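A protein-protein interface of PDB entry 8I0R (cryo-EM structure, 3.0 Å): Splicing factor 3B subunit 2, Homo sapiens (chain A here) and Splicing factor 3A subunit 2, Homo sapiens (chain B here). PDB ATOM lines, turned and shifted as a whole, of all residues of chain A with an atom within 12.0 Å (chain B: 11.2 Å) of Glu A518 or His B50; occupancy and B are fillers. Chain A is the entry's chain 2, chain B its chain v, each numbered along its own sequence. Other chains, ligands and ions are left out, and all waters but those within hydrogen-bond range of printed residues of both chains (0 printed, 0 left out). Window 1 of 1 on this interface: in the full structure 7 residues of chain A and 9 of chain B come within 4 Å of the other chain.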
ATOM      1  N   LEU A 511       5.488  -9.972 -24.979  1.00  0.00           N
ATOM      2  CA  LEU A 511       5.076  -9.745 -23.616  1.00  0.00           C
ATOM      3  C   LEU A 511       5.046 -11.049 -22.835  1.00  0.00           C
ATOM      4  O   LEU A 511       4.931 -11.041 -21.598  1.00  0.00           O
ATOM      5  CB  LEU A 511       3.778  -8.963 -23.632  1.00  0.00           C
ATOM      6  CG  LEU A 511       4.032  -7.702 -24.460  1.00  0.00           C
ATOM      7  CD1 LEU A 511       2.822  -6.893 -24.649  1.00  0.00           C
ATOM      8  CD2 LEU A 511       5.069  -6.876 -23.799  1.00  0.00           C
ATOM      9  N   GLN A 512       5.270 -12.158 -23.533  1.00  0.00           N
ATOM     10  CA  GLN A 512       5.704 -13.376 -22.873  1.00  0.00           C
ATOM     11  C   GLN A 512       6.785 -13.065 -21.858  1.00  0.00           C
ATOM     12  O   GLN A 512       6.860 -13.691 -20.800  1.00  0.00           O
ATOM     13  CB  GLN A 512       6.201 -14.366 -23.919  1.00  0.00           C
ATOM     14  CG  GLN A 512       5.098 -15.190 -24.570  1.00  0.00           C
ATOM     15  CD  GLN A 512       3.858 -14.381 -24.934  1.00  0.00           C
ATOM     16  OE1 GLN A 512       3.951 -13.253 -25.409  1.00  0.00           O
ATOM     17  NE2 GLN A 512       2.690 -14.965 -24.721  1.00  0.00           N
ATOM     18  N   GLY A 513       7.617 -12.081 -22.152  1.00  0.00           N
ATOM     19  CA  GLY A 513       8.507 -11.576 -21.135  1.00  0.00           C
ATOM     20  C   GLY A 513       7.790 -10.688 -20.144  1.00  0.00           C
ATOM     21  O   GLY A 513       8.126 -10.682 -18.957  1.00  0.00           O
ATOM     22  N   LYS A 514       6.771  -9.940 -20.603  1.00  0.00           N
ATOM     23  CA  LYS A 514       5.989  -9.144 -19.623  1.00  0.00           C
ATOM     24  C   LYS A 514       5.478  -9.974 -18.442  1.00  0.00           C
ATOM     25  O   LYS A 514       4.981  -9.432 -17.453  1.00  0.00           O
ATOM     26  CB  LYS A 514       4.791  -8.442 -20.264  1.00  0.00           C
ATOM     27  CG  LYS A 514       4.222  -7.313 -19.435  1.00  0.00           C
ATOM     28  CD  LYS A 514       2.960  -6.813 -20.056  1.00  0.00           C
ATOM     29  CE  LYS A 514       2.777  -5.345 -19.856  1.00  0.00           C
ATOM     30  NZ  LYS A 514       3.945  -4.621 -20.365  1.00  0.00           N
ATOM     31  N   ARG A 515       5.587 -11.288 -18.539  1.00  0.00           N
ATOM     32  CA  ARG A 515       4.981 -12.268 -17.630  1.00  0.00           C
ATOM     33  C   ARG A 515       4.825 -11.971 -16.133  1.00  0.00           C
ATOM     34  O   ARG A 515       3.701 -11.969 -15.634  1.00  0.00           O
ATOM     35  CB  ARG A 515       5.818 -13.547 -17.737  1.00  0.00           C
ATOM     36  CG  ARG A 515       5.626 -14.578 -16.671  1.00  0.00           C
ATOM     37  CD  ARG A 515       6.370 -15.805 -17.101  1.00  0.00           C
ATOM     38  NE  ARG A 515       6.010 -16.162 -18.466  1.00  0.00           N
ATOM     39  CZ  ARG A 515       6.048 -17.392 -18.963  1.00  0.00           C
ATOM     40  NH1 ARG A 515       6.442 -18.403 -18.218  1.00  0.00           N
ATOM     41  NH2 ARG A 515       5.699 -17.609 -20.216  1.00  0.00           N
ATOM     42  N   GLY A 516       5.914 -11.711 -15.412  1.00  0.00           N
ATOM     43  CA  GLY A 516       6.002 -12.136 -14.012  1.00  0.00           C
ATOM     44  C   GLY A 516       4.983 -11.536 -13.051  1.00  0.00           C
ATOM     45  O   GLY A 516       4.295 -12.265 -12.335  1.00  0.00           O
ATOM     46  N   ILE A 517       4.892 -10.200 -12.999  1.00  0.00           N
ATOM     47  CA  ILE A 517       4.289  -9.503 -11.845  1.00  0.00           C
ATOM     48  C   ILE A 517       2.765  -9.477 -11.924  1.00  0.00           C
ATOM     49  O   ILE A 517       2.149  -9.862 -12.919  1.00  0.00           O
ATOM     50  CB  ILE A 517       4.856  -8.082 -11.708  1.00  0.00           C
ATOM     51  CG1 ILE A 517       5.211  -7.496 -13.078  1.00  0.00           C
ATOM     52  CG2 ILE A 517       6.052  -8.084 -10.792  1.00  0.00           C
ATOM     53  CD1 ILE A 517       4.026  -7.227 -13.981  1.00  0.00           C
ATOM     54  N   GLU A 518       2.153  -9.014 -10.833  1.00  0.00           N
ATOM     55  CA  GLU A 518       0.700  -8.890 -10.733  1.00  0.00           C
ATOM     56  C   GLU A 518       0.252  -7.465 -11.050  1.00  0.00           C
ATOM     57  O   GLU A 518       1.006  -6.506 -10.864  1.00  0.00           O
ATOM     58  CB  GLU A 518       0.243  -9.298  -9.330  1.00  0.00           C
ATOM     59  CG  GLU A 518      -1.147  -8.855  -8.901  1.00  0.00           C
ATOM     60  CD  GLU A 518      -2.259  -9.481  -9.715  1.00  0.00           C
ATOM     61  OE1 GLU A 518      -2.360  -9.190 -10.921  1.00  0.00           O
ATOM     62  OE2 GLU A 518      -3.047 -10.265  -9.145  1.00  0.00           O
ATOM     63  N   LYS A 519      -0.992  -7.329 -11.529  1.00  0.00           N
ATOM     64  CA  LYS A 519      -1.509  -6.134 -12.177  1.00  0.00           C
ATOM     65  C   LYS A 519      -2.876  -5.741 -11.624  1.00  0.00           C
ATOM     66  O   LYS A 519      -3.707  -6.613 -11.363  1.00  0.00           O
ATOM     67  CB  LYS A 519      -1.621  -6.383 -13.683  1.00  0.00           C
ATOM     68  CG  LYS A 519      -2.111  -5.214 -14.481  1.00  0.00           C
ATOM     69  CD  LYS A 519      -2.748  -5.667 -15.768  1.00  0.00           C
ATOM     70  CE  LYS A 519      -4.024  -4.905 -16.012  1.00  0.00           C
ATOM     71  NZ  LYS A 519      -3.807  -3.454 -15.783  1.00  0.00           N
ATOM     72  N   PRO A 520      -3.146  -4.443 -11.448  1.00  0.00           N
ATOM     73  CA  PRO A 520      -4.457  -4.033 -10.953  1.00  0.00           C
ATOM     74  C   PRO A 520      -5.464  -3.956 -12.086  1.00  0.00           C
ATOM     75  O   PRO A 520      -5.110  -3.610 -13.225  1.00  0.00           O
ATOM     76  CB  PRO A 520      -4.188  -2.643 -10.358  1.00  0.00           C
ATOM     77  CG  PRO A 520      -3.129  -2.118 -11.237  1.00  0.00           C
ATOM     78  CD  PRO A 520      -2.241  -3.289 -11.584  1.00  0.00           C
ATOM     79  N   PRO A 521      -6.734  -4.253 -11.816  1.00  0.00           N
ATOM     80  CA  PRO A 521      -7.740  -4.249 -12.881  1.00  0.00           C
ATOM     81  C   PRO A 521      -7.851  -2.904 -13.578  1.00  0.00           C
ATOM     82  O   PRO A 521      -7.467  -1.865 -13.042  1.00  0.00           O
ATOM     83  CB  PRO A 521      -9.036  -4.594 -12.143  1.00  0.00           C
ATOM     84  CG  PRO A 521      -8.722  -4.492 -10.710  1.00  0.00           C
ATOM     85  CD  PRO A 521      -7.281  -4.779 -10.564  1.00  0.00           C
ATOM     86  N   PHE A 522      -8.382  -2.949 -14.799  1.00  0.00           N
ATOM     87  CA  PHE A 522      -8.594  -1.761 -15.610  1.00  0.00           C
ATOM     88  C   PHE A 522      -9.280  -0.685 -14.792  1.00  0.00           C
ATOM     89  O   PHE A 522     -10.023  -0.976 -13.858  1.00  0.00           O
ATOM     90  CB  PHE A 522      -9.428  -2.140 -16.835  1.00  0.00           C
ATOM     91  CG  PHE A 522      -9.926  -0.980 -17.634  1.00  0.00           C
ATOM     92  CD1 PHE A 522     -11.258  -0.874 -17.951  1.00  0.00           C
ATOM     93  CD2 PHE A 522      -9.063  -0.021 -18.099  1.00  0.00           C
ATOM     94  CE1 PHE A 522     -11.716   0.174 -18.683  1.00  0.00           C
ATOM     95  CE2 PHE A 522      -9.528   1.026 -18.830  1.00  0.00           C
ATOM     96  CZ  PHE A 522     -10.853   1.121 -19.125  1.00  0.00           C
ATOM     97  N   GLU A 523      -8.996   0.566 -15.118  1.00  0.00           N
ATOM     98  CA  GLU A 523      -9.475   1.703 -14.350  1.00  0.00           C
ATOM     99  C   GLU A 523     -10.385   2.558 -15.216  1.00  0.00           C
ATOM    100  O   GLU A 523      -9.943   3.114 -16.222  1.00  0.00           O
ATOM    101  CB  GLU A 523      -8.294   2.519 -13.849  1.00  0.00           C
ATOM    102  CG  GLU A 523      -8.645   3.923 -13.516  1.00  0.00           C
ATOM    103  CD  GLU A 523      -8.913   4.087 -12.053  1.00  0.00           C
ATOM    104  OE1 GLU A 523      -9.589   5.064 -11.680  1.00  0.00           O
ATOM    105  OE2 GLU A 523      -8.446   3.232 -11.274  1.00  0.00           O
ATOM    106  N   TYR A 591       5.349   1.391 -28.324  1.00  0.00           N
ATOM    107  CA  TYR A 591       5.354   0.832 -26.993  1.00  0.00           C
ATOM    108  C   TYR A 591       6.259  -0.386 -26.949  1.00  0.00           C
ATOM    109  O   TYR A 591       6.418  -1.093 -27.941  1.00  0.00           O
ATOM    110  CB  TYR A 591       3.938   0.469 -26.587  1.00  0.00           C
ATOM    111  CG  TYR A 591       3.834  -0.262 -25.290  1.00  0.00           C
ATOM    112  CD1 TYR A 591       3.749  -1.629 -25.258  1.00  0.00           C
ATOM    113  CD2 TYR A 591       3.797   0.417 -24.098  1.00  0.00           C
ATOM    114  CE1 TYR A 591       3.651  -2.293 -24.078  1.00  0.00           C
ATOM    115  CE2 TYR A 591       3.691  -0.243 -22.927  1.00  0.00           C
ATOM    116  CZ  TYR A 591       3.623  -1.592 -22.918  1.00  0.00           C
ATOM    117  OH  TYR A 591       3.525  -2.242 -21.726  1.00  0.00           O
ATOM    118  N   GLU A 593       8.012  -3.462 -23.901  1.00  0.00           N
ATOM    119  CA  GLU A 593       7.812  -4.024 -22.579  1.00  0.00           C
ATOM    120  C   GLU A 593       8.489  -3.177 -21.519  1.00  0.00           C
ATOM    121  O   GLU A 593       9.716  -3.074 -21.493  1.00  0.00           O
ATOM    122  CB  GLU A 593       8.357  -5.432 -22.501  1.00  0.00           C
ATOM    123  CG  GLU A 593       7.976  -6.094 -21.232  1.00  0.00           C
ATOM    124  CD  GLU A 593       8.500  -7.485 -21.150  1.00  0.00           C
ATOM    125  OE1 GLU A 593       8.595  -8.153 -22.193  1.00  0.00           O
ATOM    126  OE2 GLU A 593       8.827  -7.912 -20.028  1.00  0.00           O
ATOM    127  N   GLU A 596       5.703   1.560 -19.366  1.00  0.00           N
ATOM    128  CA  GLU A 596       4.788   2.169 -18.417  1.00  0.00           C
ATOM    129  C   GLU A 596       5.336   2.172 -17.006  1.00  0.00           C
ATOM    130  O   GLU A 596       4.620   2.559 -16.081  1.00  0.00           O
ATOM    131  CB  GLU A 596       3.448   1.439 -18.442  1.00  0.00           C
ATOM    132  CG  GLU A 596       3.476   0.086 -17.785  1.00  0.00           C
ATOM    133  CD  GLU A 596       4.072  -0.996 -18.657  1.00  0.00           C
ATOM    134  OE1 GLU A 596       3.389  -2.012 -18.879  1.00  0.00           O
ATOM    135  OE2 GLU A 596       5.227  -0.849 -19.106  1.00  0.00           O
ATOM    136  N   PHE A 597       6.573   1.741 -16.819  1.00  0.00           N
ATOM    137  CA  PHE A 597       7.219   1.809 -15.522  1.00  0.00           C
ATOM    138  C   PHE A 597       8.438   2.697 -15.663  1.00  0.00           C
ATOM    139  O   PHE A 597       9.518   2.388 -15.154  1.00  0.00           O
ATOM    140  CB  PHE A 597       7.593   0.418 -15.026  1.00  0.00           C
ATOM    141  CG  PHE A 597       6.416  -0.473 -14.820  1.00  0.00           C
ATOM    142  CD1 PHE A 597       5.268   0.013 -14.238  1.00  0.00           C
ATOM    143  CD2 PHE A 597       6.443  -1.788 -15.231  1.00  0.00           C
ATOM    144  CE1 PHE A 597       4.175  -0.800 -14.051  1.00  0.00           C
ATOM    145  CE2 PHE A 597       5.348  -2.602 -15.048  1.00  0.00           C
ATOM    146  CZ  PHE A 597       4.216  -2.106 -14.455  1.00  0.00           C
ATOM    147  N   ARG B  31     -11.810 -24.481  -8.059  1.00  0.00           N
ATOM    148  CA  ARG B  31     -10.951 -23.364  -7.695  1.00  0.00           C
ATOM    149  C   ARG B  31     -10.890 -23.187  -6.189  1.00  0.00           C
ATOM    150  O   ARG B  31      -9.815 -22.966  -5.617  1.00  0.00           O
ATOM    151  CB  ARG B  31     -11.446 -22.092  -8.358  1.00  0.00           C
ATOM    152  CG  ARG B  31     -11.018 -20.848  -7.641  1.00  0.00           C
ATOM    153  CD  ARG B  31     -11.425 -19.622  -8.402  1.00  0.00           C
ATOM    154  NE  ARG B  31     -11.739 -19.914  -9.795  1.00  0.00           N
ATOM    155  CZ  ARG B  31     -12.936 -19.735 -10.346  1.00  0.00           C
ATOM    156  NH1 ARG B  31     -13.939 -19.255  -9.624  1.00  0.00           N
ATOM    157  NH2 ARG B  31     -13.131 -20.028 -11.624  1.00  0.00           N
ATOM    158  N   PHE B  46       2.580 -19.087  -4.694  1.00  0.00           N
ATOM    159  CA  PHE B  46       1.541 -19.222  -5.699  1.00  0.00           C
ATOM    160  C   PHE B  46       0.801 -17.906  -5.805  1.00  0.00           C
ATOM    161  O   PHE B  46       0.626 -17.214  -4.802  1.00  0.00           O
ATOM    162  CB  PHE B  46       0.626 -20.384  -5.329  1.00  0.00           C
ATOM    163  CG  PHE B  46      -0.821 -20.167  -5.595  1.00  0.00           C
ATOM    164  CD1 PHE B  46      -1.600 -19.399  -4.764  1.00  0.00           C
ATOM    165  CD2 PHE B  46      -1.428 -20.821  -6.638  1.00  0.00           C
ATOM    166  CE1 PHE B  46      -2.930 -19.242  -5.014  1.00  0.00           C
ATOM    167  CE2 PHE B  46      -2.761 -20.675  -6.879  1.00  0.00           C
ATOM    168  CZ  PHE B  46      -3.512 -19.886  -6.066  1.00  0.00           C
ATOM    169  N   MET B  47       0.395 -17.544  -7.013  1.00  0.00           N
ATOM    170  CA  MET B  47      -0.358 -16.314  -7.183  1.00  0.00           C
ATOM    171  C   MET B  47      -1.398 -16.488  -8.271  1.00  0.00           C
ATOM    172  O   MET B  47      -1.228 -17.294  -9.182  1.00  0.00           O
ATOM    173  CB  MET B  47       0.550 -15.135  -7.524  1.00  0.00           C
ATOM    174  CG  MET B  47       0.386 -14.627  -8.935  1.00  0.00           C
ATOM    175  SD  MET B  47       1.341 -13.161  -9.279  1.00  0.00           S
ATOM    176  CE  MET B  47       1.618 -12.562  -7.623  1.00  0.00           C
ATOM    177  N   LYS B  48      -2.475 -15.734  -8.157  1.00  0.00           N
ATOM    178  CA  LYS B  48      -3.516 -15.679  -9.165  1.00  0.00           C
ATOM    179  C   LYS B  48      -3.362 -14.384  -9.941  1.00  0.00           C
ATOM    180  O   LYS B  48      -3.375 -13.304  -9.346  1.00  0.00           O
ATOM    181  CB  LYS B  48      -4.884 -15.739  -8.509  1.00  0.00           C
ATOM    182  CG  LYS B  48      -5.996 -16.008  -9.463  1.00  0.00           C
ATOM    183  CD  LYS B  48      -7.294 -16.122  -8.721  1.00  0.00           C
ATOM    184  CE  LYS B  48      -8.187 -17.151  -9.352  1.00  0.00           C
ATOM    185  NZ  LYS B  48      -9.418 -17.291  -8.558  1.00  0.00           N
ATOM    186  N   ASN B  49      -3.224 -14.480 -11.257  1.00  0.00           N
ATOM    187  CA  ASN B  49      -3.073 -13.264 -12.033  1.00  0.00           C
ATOM    188  C   ASN B  49      -4.429 -12.777 -12.518  1.00  0.00           C
ATOM    189  O   ASN B  49      -5.462 -13.410 -12.314  1.00  0.00           O
ATOM    190  CB  ASN B  49      -2.132 -13.481 -13.205  1.00  0.00           C
ATOM    191  CG  ASN B  49      -2.523 -14.644 -14.031  1.00  0.00           C
ATOM    192  OD1 ASN B  49      -3.440 -15.363 -13.692  1.00  0.00           O
ATOM    193  ND2 ASN B  49      -1.826 -14.852 -15.126  1.00  0.00           N
ATOM    194  N   HIS B  50      -4.417 -11.623 -13.173  1.00  0.00           N
ATOM    195  CA  HIS B  50      -5.664 -10.934 -13.470  1.00  0.00           C
ATOM    196  C   HIS B  50      -6.461 -11.595 -14.579  1.00  0.00           C
ATOM    197  O   HIS B  50      -7.481 -11.049 -14.993  1.00  0.00           O
ATOM    198  CB  HIS B  50      -5.382  -9.486 -13.837  1.00  0.00           C
ATOM    199  CG  HIS B  50      -4.585  -9.329 -15.085  1.00  0.00           C
ATOM    200  ND1 HIS B  50      -3.612 -10.222 -15.464  1.00  0.00           N
ATOM    201  CD2 HIS B  50      -4.638  -8.393 -16.058  1.00  0.00           C
ATOM    202  CE1 HIS B  50      -3.086  -9.837 -16.612  1.00  0.00           C
ATOM    203  NE2 HIS B  50      -3.690  -8.728 -16.991  1.00  0.00           N
ATOM    204  N   LEU B  51      -6.028 -12.739 -15.078  1.00  0.00           N
ATOM    205  CA  LEU B  51      -6.858 -13.501 -15.987  1.00  0.00           C
ATOM    206  C   LEU B  51      -7.378 -14.770 -15.363  1.00  0.00           C
ATOM    207  O   LEU B  51      -7.895 -15.627 -16.081  1.00  0.00           O
ATOM    208  CB  LEU B  51      -6.099 -13.854 -17.251  1.00  0.00           C
ATOM    209  CG  LEU B  51      -5.389 -12.695 -17.908  1.00  0.00           C
ATOM    210  CD1 LEU B  51      -3.903 -12.922 -17.857  1.00  0.00           C
ATOM    211  CD2 LEU B  51      -5.864 -12.580 -19.301  1.00  0.00           C
ATOM    212  N   GLY B  52      -7.255 -14.921 -14.057  1.00  0.00           N
ATOM    213  CA  GLY B  52      -7.803 -16.076 -13.400  1.00  0.00           C
ATOM    214  C   GLY B  52      -7.059 -17.360 -13.645  1.00  0.00           C
ATOM    215  O   GLY B  52      -7.626 -18.434 -13.435  1.00  0.00           O
ATOM    216  N   SER B  53      -5.828 -17.288 -14.110  1.00  0.00           N
ATOM    217  CA  SER B  53      -4.975 -18.450 -14.138  1.00  0.00           C
ATOM    218  C   SER B  53      -3.964 -18.292 -13.021  1.00  0.00           C
ATOM    219  O   SER B  53      -4.059 -17.375 -12.211  1.00  0.00           O
ATOM    220  CB  SER B  53      -4.293 -18.596 -15.491  1.00  0.00           C
ATOM    221  OG  SER B  53      -3.319 -17.591 -15.675  1.00  0.00           O
ATOM    222  N   TYR B  54      -3.009 -19.200 -12.946  1.00  0.00           N
ATOM    223  CA  TYR B  54      -2.124 -19.209 -11.798  1.00  0.00           C
ATOM    224  C   TYR B  54      -0.686 -19.065 -12.235  1.00  0.00           C
ATOM    225  O   TYR B  54      -0.352 -19.350 -13.383  1.00  0.00           O
ATOM    226  CB  TYR B  54      -2.328 -20.482 -10.999  1.00  0.00           C
ATOM    227  CG  TYR B  54      -3.781 -20.690 -10.748  1.00  0.00           C
ATOM    228  CD1 TYR B  54      -4.425 -19.988  -9.757  1.00  0.00           C
ATOM    229  CD2 TYR B  54      -4.521 -21.535 -11.536  1.00  0.00           C
ATOM    230  CE1 TYR B  54      -5.753 -20.155  -9.534  1.00  0.00           C
ATOM    231  CE2 TYR B  54      -5.843 -21.698 -11.325  1.00  0.00           C
ATOM    232  CZ  TYR B  54      -6.453 -21.008 -10.321  1.00  0.00           C
ATOM    233  OH  TYR B  54      -7.787 -21.172 -10.101  1.00  0.00           O
ATOM    234  N   GLU B  55       0.152 -18.607 -11.326  1.00  0.00           N
ATOM    235  CA  GLU B  55       1.567 -18.452 -11.575  1.00  0.00           C
ATOM    236  C   GLU B  55       2.338 -18.973 -10.386  1.00  0.00           C
ATOM    237  O   GLU B  55       1.888 -18.849  -9.245  1.00  0.00           O
ATOM    238  CB  GLU B  55       1.912 -17.004 -11.802  1.00  0.00           C
ATOM    239  CG  GLU B  55       1.408 -16.510 -13.103  1.00  0.00           C
ATOM    240  CD  GLU B  55       1.218 -15.030 -13.115  1.00  0.00           C
ATOM    241  OE1 GLU B  55       0.730 -14.505 -14.128  1.00  0.00           O
ATOM    242  OE2 GLU B  55       1.553 -14.387 -12.107  1.00  0.00           O
ATOM    243  N   CYS B  56       3.500 -19.538 -10.655  1.00  0.00           N
ATOM    244  CA  CYS B  56       4.442 -19.890  -9.605  1.00  0.00           C
ATOM    245  C   CYS B  56       5.430 -18.746  -9.472  1.00  0.00           C
ATOM    246  O   CYS B  56       6.324 -18.594 -10.302  1.00  0.00           O
ATOM    247  CB  CYS B  56       5.161 -21.192  -9.915  1.00  0.00           C
ATOM    248  SG  CYS B  56       5.978 -21.929  -8.507  1.00  0.00           S
ATOM    249  N   LYS B  57       5.277 -17.953  -8.418  1.00  0.00           N
ATOM    250  CA  LYS B  57       6.134 -16.795  -8.215  1.00  0.00           C
ATOM    251  C   LYS B  57       7.597 -17.177  -8.070  1.00  0.00           C
ATOM    252  O   LYS B  57       8.464 -16.300  -8.070  1.00  0.00           O
ATOM    253  CB  LYS B  57       5.685 -16.036  -6.975  1.00  0.00           C
ATOM    254  CG  LYS B  57       4.933 -14.775  -7.271  1.00  0.00           C
ATOM    255  CD  LYS B  57       4.606 -14.027  -6.005  1.00  0.00           C
ATOM    256  CE  LYS B  57       3.593 -14.760  -5.169  1.00  0.00           C
ATOM    257  NZ  LYS B  57       3.378 -14.059  -3.885  1.00  0.00           N
ATOM    258  N   LEU B  60       8.381 -19.054 -11.955  1.00  0.00           N
ATOM    259  CA  LEU B  60       7.933 -18.091 -12.960  1.00  0.00           C
ATOM    260  C   LEU B  60       7.264 -18.785 -14.134  1.00  0.00           C
ATOM    261  O   LEU B  60       7.537 -18.489 -15.291  1.00  0.00           O
ATOM    262  CB  LEU B  60       9.082 -17.211 -13.439  1.00  0.00           C
ATOM    263  CG  LEU B  60       9.354 -15.991 -12.574  1.00  0.00           C
ATOM    264  CD1 LEU B  60      10.044 -14.944 -13.389  1.00  0.00           C
ATOM    265  CD2 LEU B  60       8.078 -15.453 -11.996  1.00  0.00           C
ATOM    266  N   THR B  61       6.373 -19.717 -13.829  1.00  0.00           N
ATOM    267  CA  THR B  61       5.609 -20.423 -14.844  1.00  0.00           C
ATOM    268  C   THR B  61       4.136 -20.090 -14.706  1.00  0.00           C
ATOM    269  O   THR B  61       3.689 -19.655 -13.643  1.00  0.00           O
ATOM    270  CB  THR B  61       5.782 -21.914 -14.725  1.00  0.00           C
ATOM    271  OG1 THR B  61       5.163 -22.344 -13.520  1.00  0.00           O
ATOM    272  CG2 THR B  61       7.222 -22.269 -14.671  1.00  0.00           C
ATOM    273  N   LEU B  62       3.387 -20.350 -15.772  1.00  0.00           N
ATOM    274  CA  LEU B  62       1.964 -20.065 -15.844  1.00  0.00           C
ATOM    275  C   LEU B  62       1.178 -21.349 -15.971  1.00  0.00           C
ATOM    276  O   LEU B  62       1.609 -22.282 -16.641  1.00  0.00           O
ATOM    277  CB  LEU B  62       1.651 -19.193 -17.044  1.00  0.00           C
ATOM    278  CG  LEU B  62       2.438 -17.913 -17.134  1.00  0.00           C
ATOM    279  CD1 LEU B  62       2.723 -17.659 -18.563  1.00  0.00           C
ATOM    280  CD2 LEU B  62       1.613 -16.809 -16.578  1.00  0.00           C
ATOM    281  N   HIS B  63       0.002 -21.379 -15.359  1.00  0.00           N
ATOM    282  CA  HIS B  63      -0.794 -22.589 -15.292  1.00  0.00           C
ATOM    283  C   HIS B  63      -2.245 -22.289 -15.599  1.00  0.00           C
ATOM    284  O   HIS B  63      -2.805 -21.321 -15.083  1.00  0.00           O
ATOM    285  CB  HIS B  63      -0.673 -23.216 -13.925  1.00  0.00           C
ATOM    286  CG  HIS B  63       0.735 -23.460 -13.508  1.00  0.00           C
ATOM    287  ND1 HIS B  63       1.576 -24.297 -14.200  1.00  0.00           N
ATOM    288  CD2 HIS B  63       1.452 -22.976 -12.476  1.00  0.00           C
ATOM    289  CE1 HIS B  63       2.752 -24.322 -13.609  1.00  0.00           C
ATOM    290  NE2 HIS B  63       2.704 -23.523 -12.564  1.00  0.00           N
ATOM    291  N   ASN B  64      -2.849 -23.149 -16.412  1.00  0.00           N
ATOM    292  CA  ASN B  64      -4.248 -23.029 -16.785  1.00  0.00           C
ATOM    293  C   ASN B  64      -5.156 -23.468 -15.656  1.00  0.00           C
ATOM    294  O   ASN B  64      -6.076 -22.741 -15.283  1.00  0.00           O
ATOM    295  CB  ASN B  64      -4.545 -23.879 -18.008  1.00  0.00           C
ATOM    296  CG  ASN B  64      -3.655 -23.571 -19.144  1.00  0.00           C
ATOM    297  OD1 ASN B  64      -3.157 -22.461 -19.266  1.00  0.00           O
ATOM    298  ND2 ASN B  64      -3.431 -24.551 -19.993  1.00  0.00           N
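The guanidinium group of Arg A515 is in hydrogen-bond range of the backbone carbonyl oxygen of Leu B60, at 3.1 Å.
O of Lys B48 lies close to OE2 of Glu A518 (3.1 Å).
The backbone carbonyl oxygen (O) of Gly A516 lies close to the side-chain carboxylate (OE2) of Glu B55, at 3.5 Å.
The backbone carbonyl oxygen (O) of Met B47 sits at hydrogen-bond distance from the backbone NH (N) of Glu B55 (2.9 Å).
OE1 of Glu B55 sits at hydrogen-bond distance from ND2 of Asn B49 (2.8 Å).
Arg A515 touches Leu B62.
CB of Glu A518 touches CE of Met B47, at 3.9 Å.
Glu A518 touches His B50 (OE1 to N, 3.9 Å).
Lys A519 touches His B50.
Of chain B, only Glu B55 (3.5 Å) comes within 4 Å of Gly A516.
Glu A518 touches just these residues of chain B: Met B47, Lys B48 and His B50.
Of the printed residues of chain B, Lys A519 touches His B50.
Of the printed residues of chain A, Met B47 touches Glu A518.
No residue of chain A comes within 4 Å of Leu B51.
Ser B53 touches none of the printed residues of chain A.
Of the printed residues of chain A, Leu B62 touches Arg A515 (3.4 Å).
The nearest residue of chain B that does not touch Glu A518 is Asn B49 (4.2 Å).
The nearest residue of chain A that does not touch His B50 is Pro A520 (5.6 Å).
The nearest printed residue of chain A that does not touch Leu B60 is Gly A516 (4.4 Å).
Along chain A the printed residues that touch a printed residue of chain B span positions 515 to 519.
Of the 18 printed residues of chain B, 6 touch a printed residue of chain A.
Among the printed residues, 7 pairs touch across the chains.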
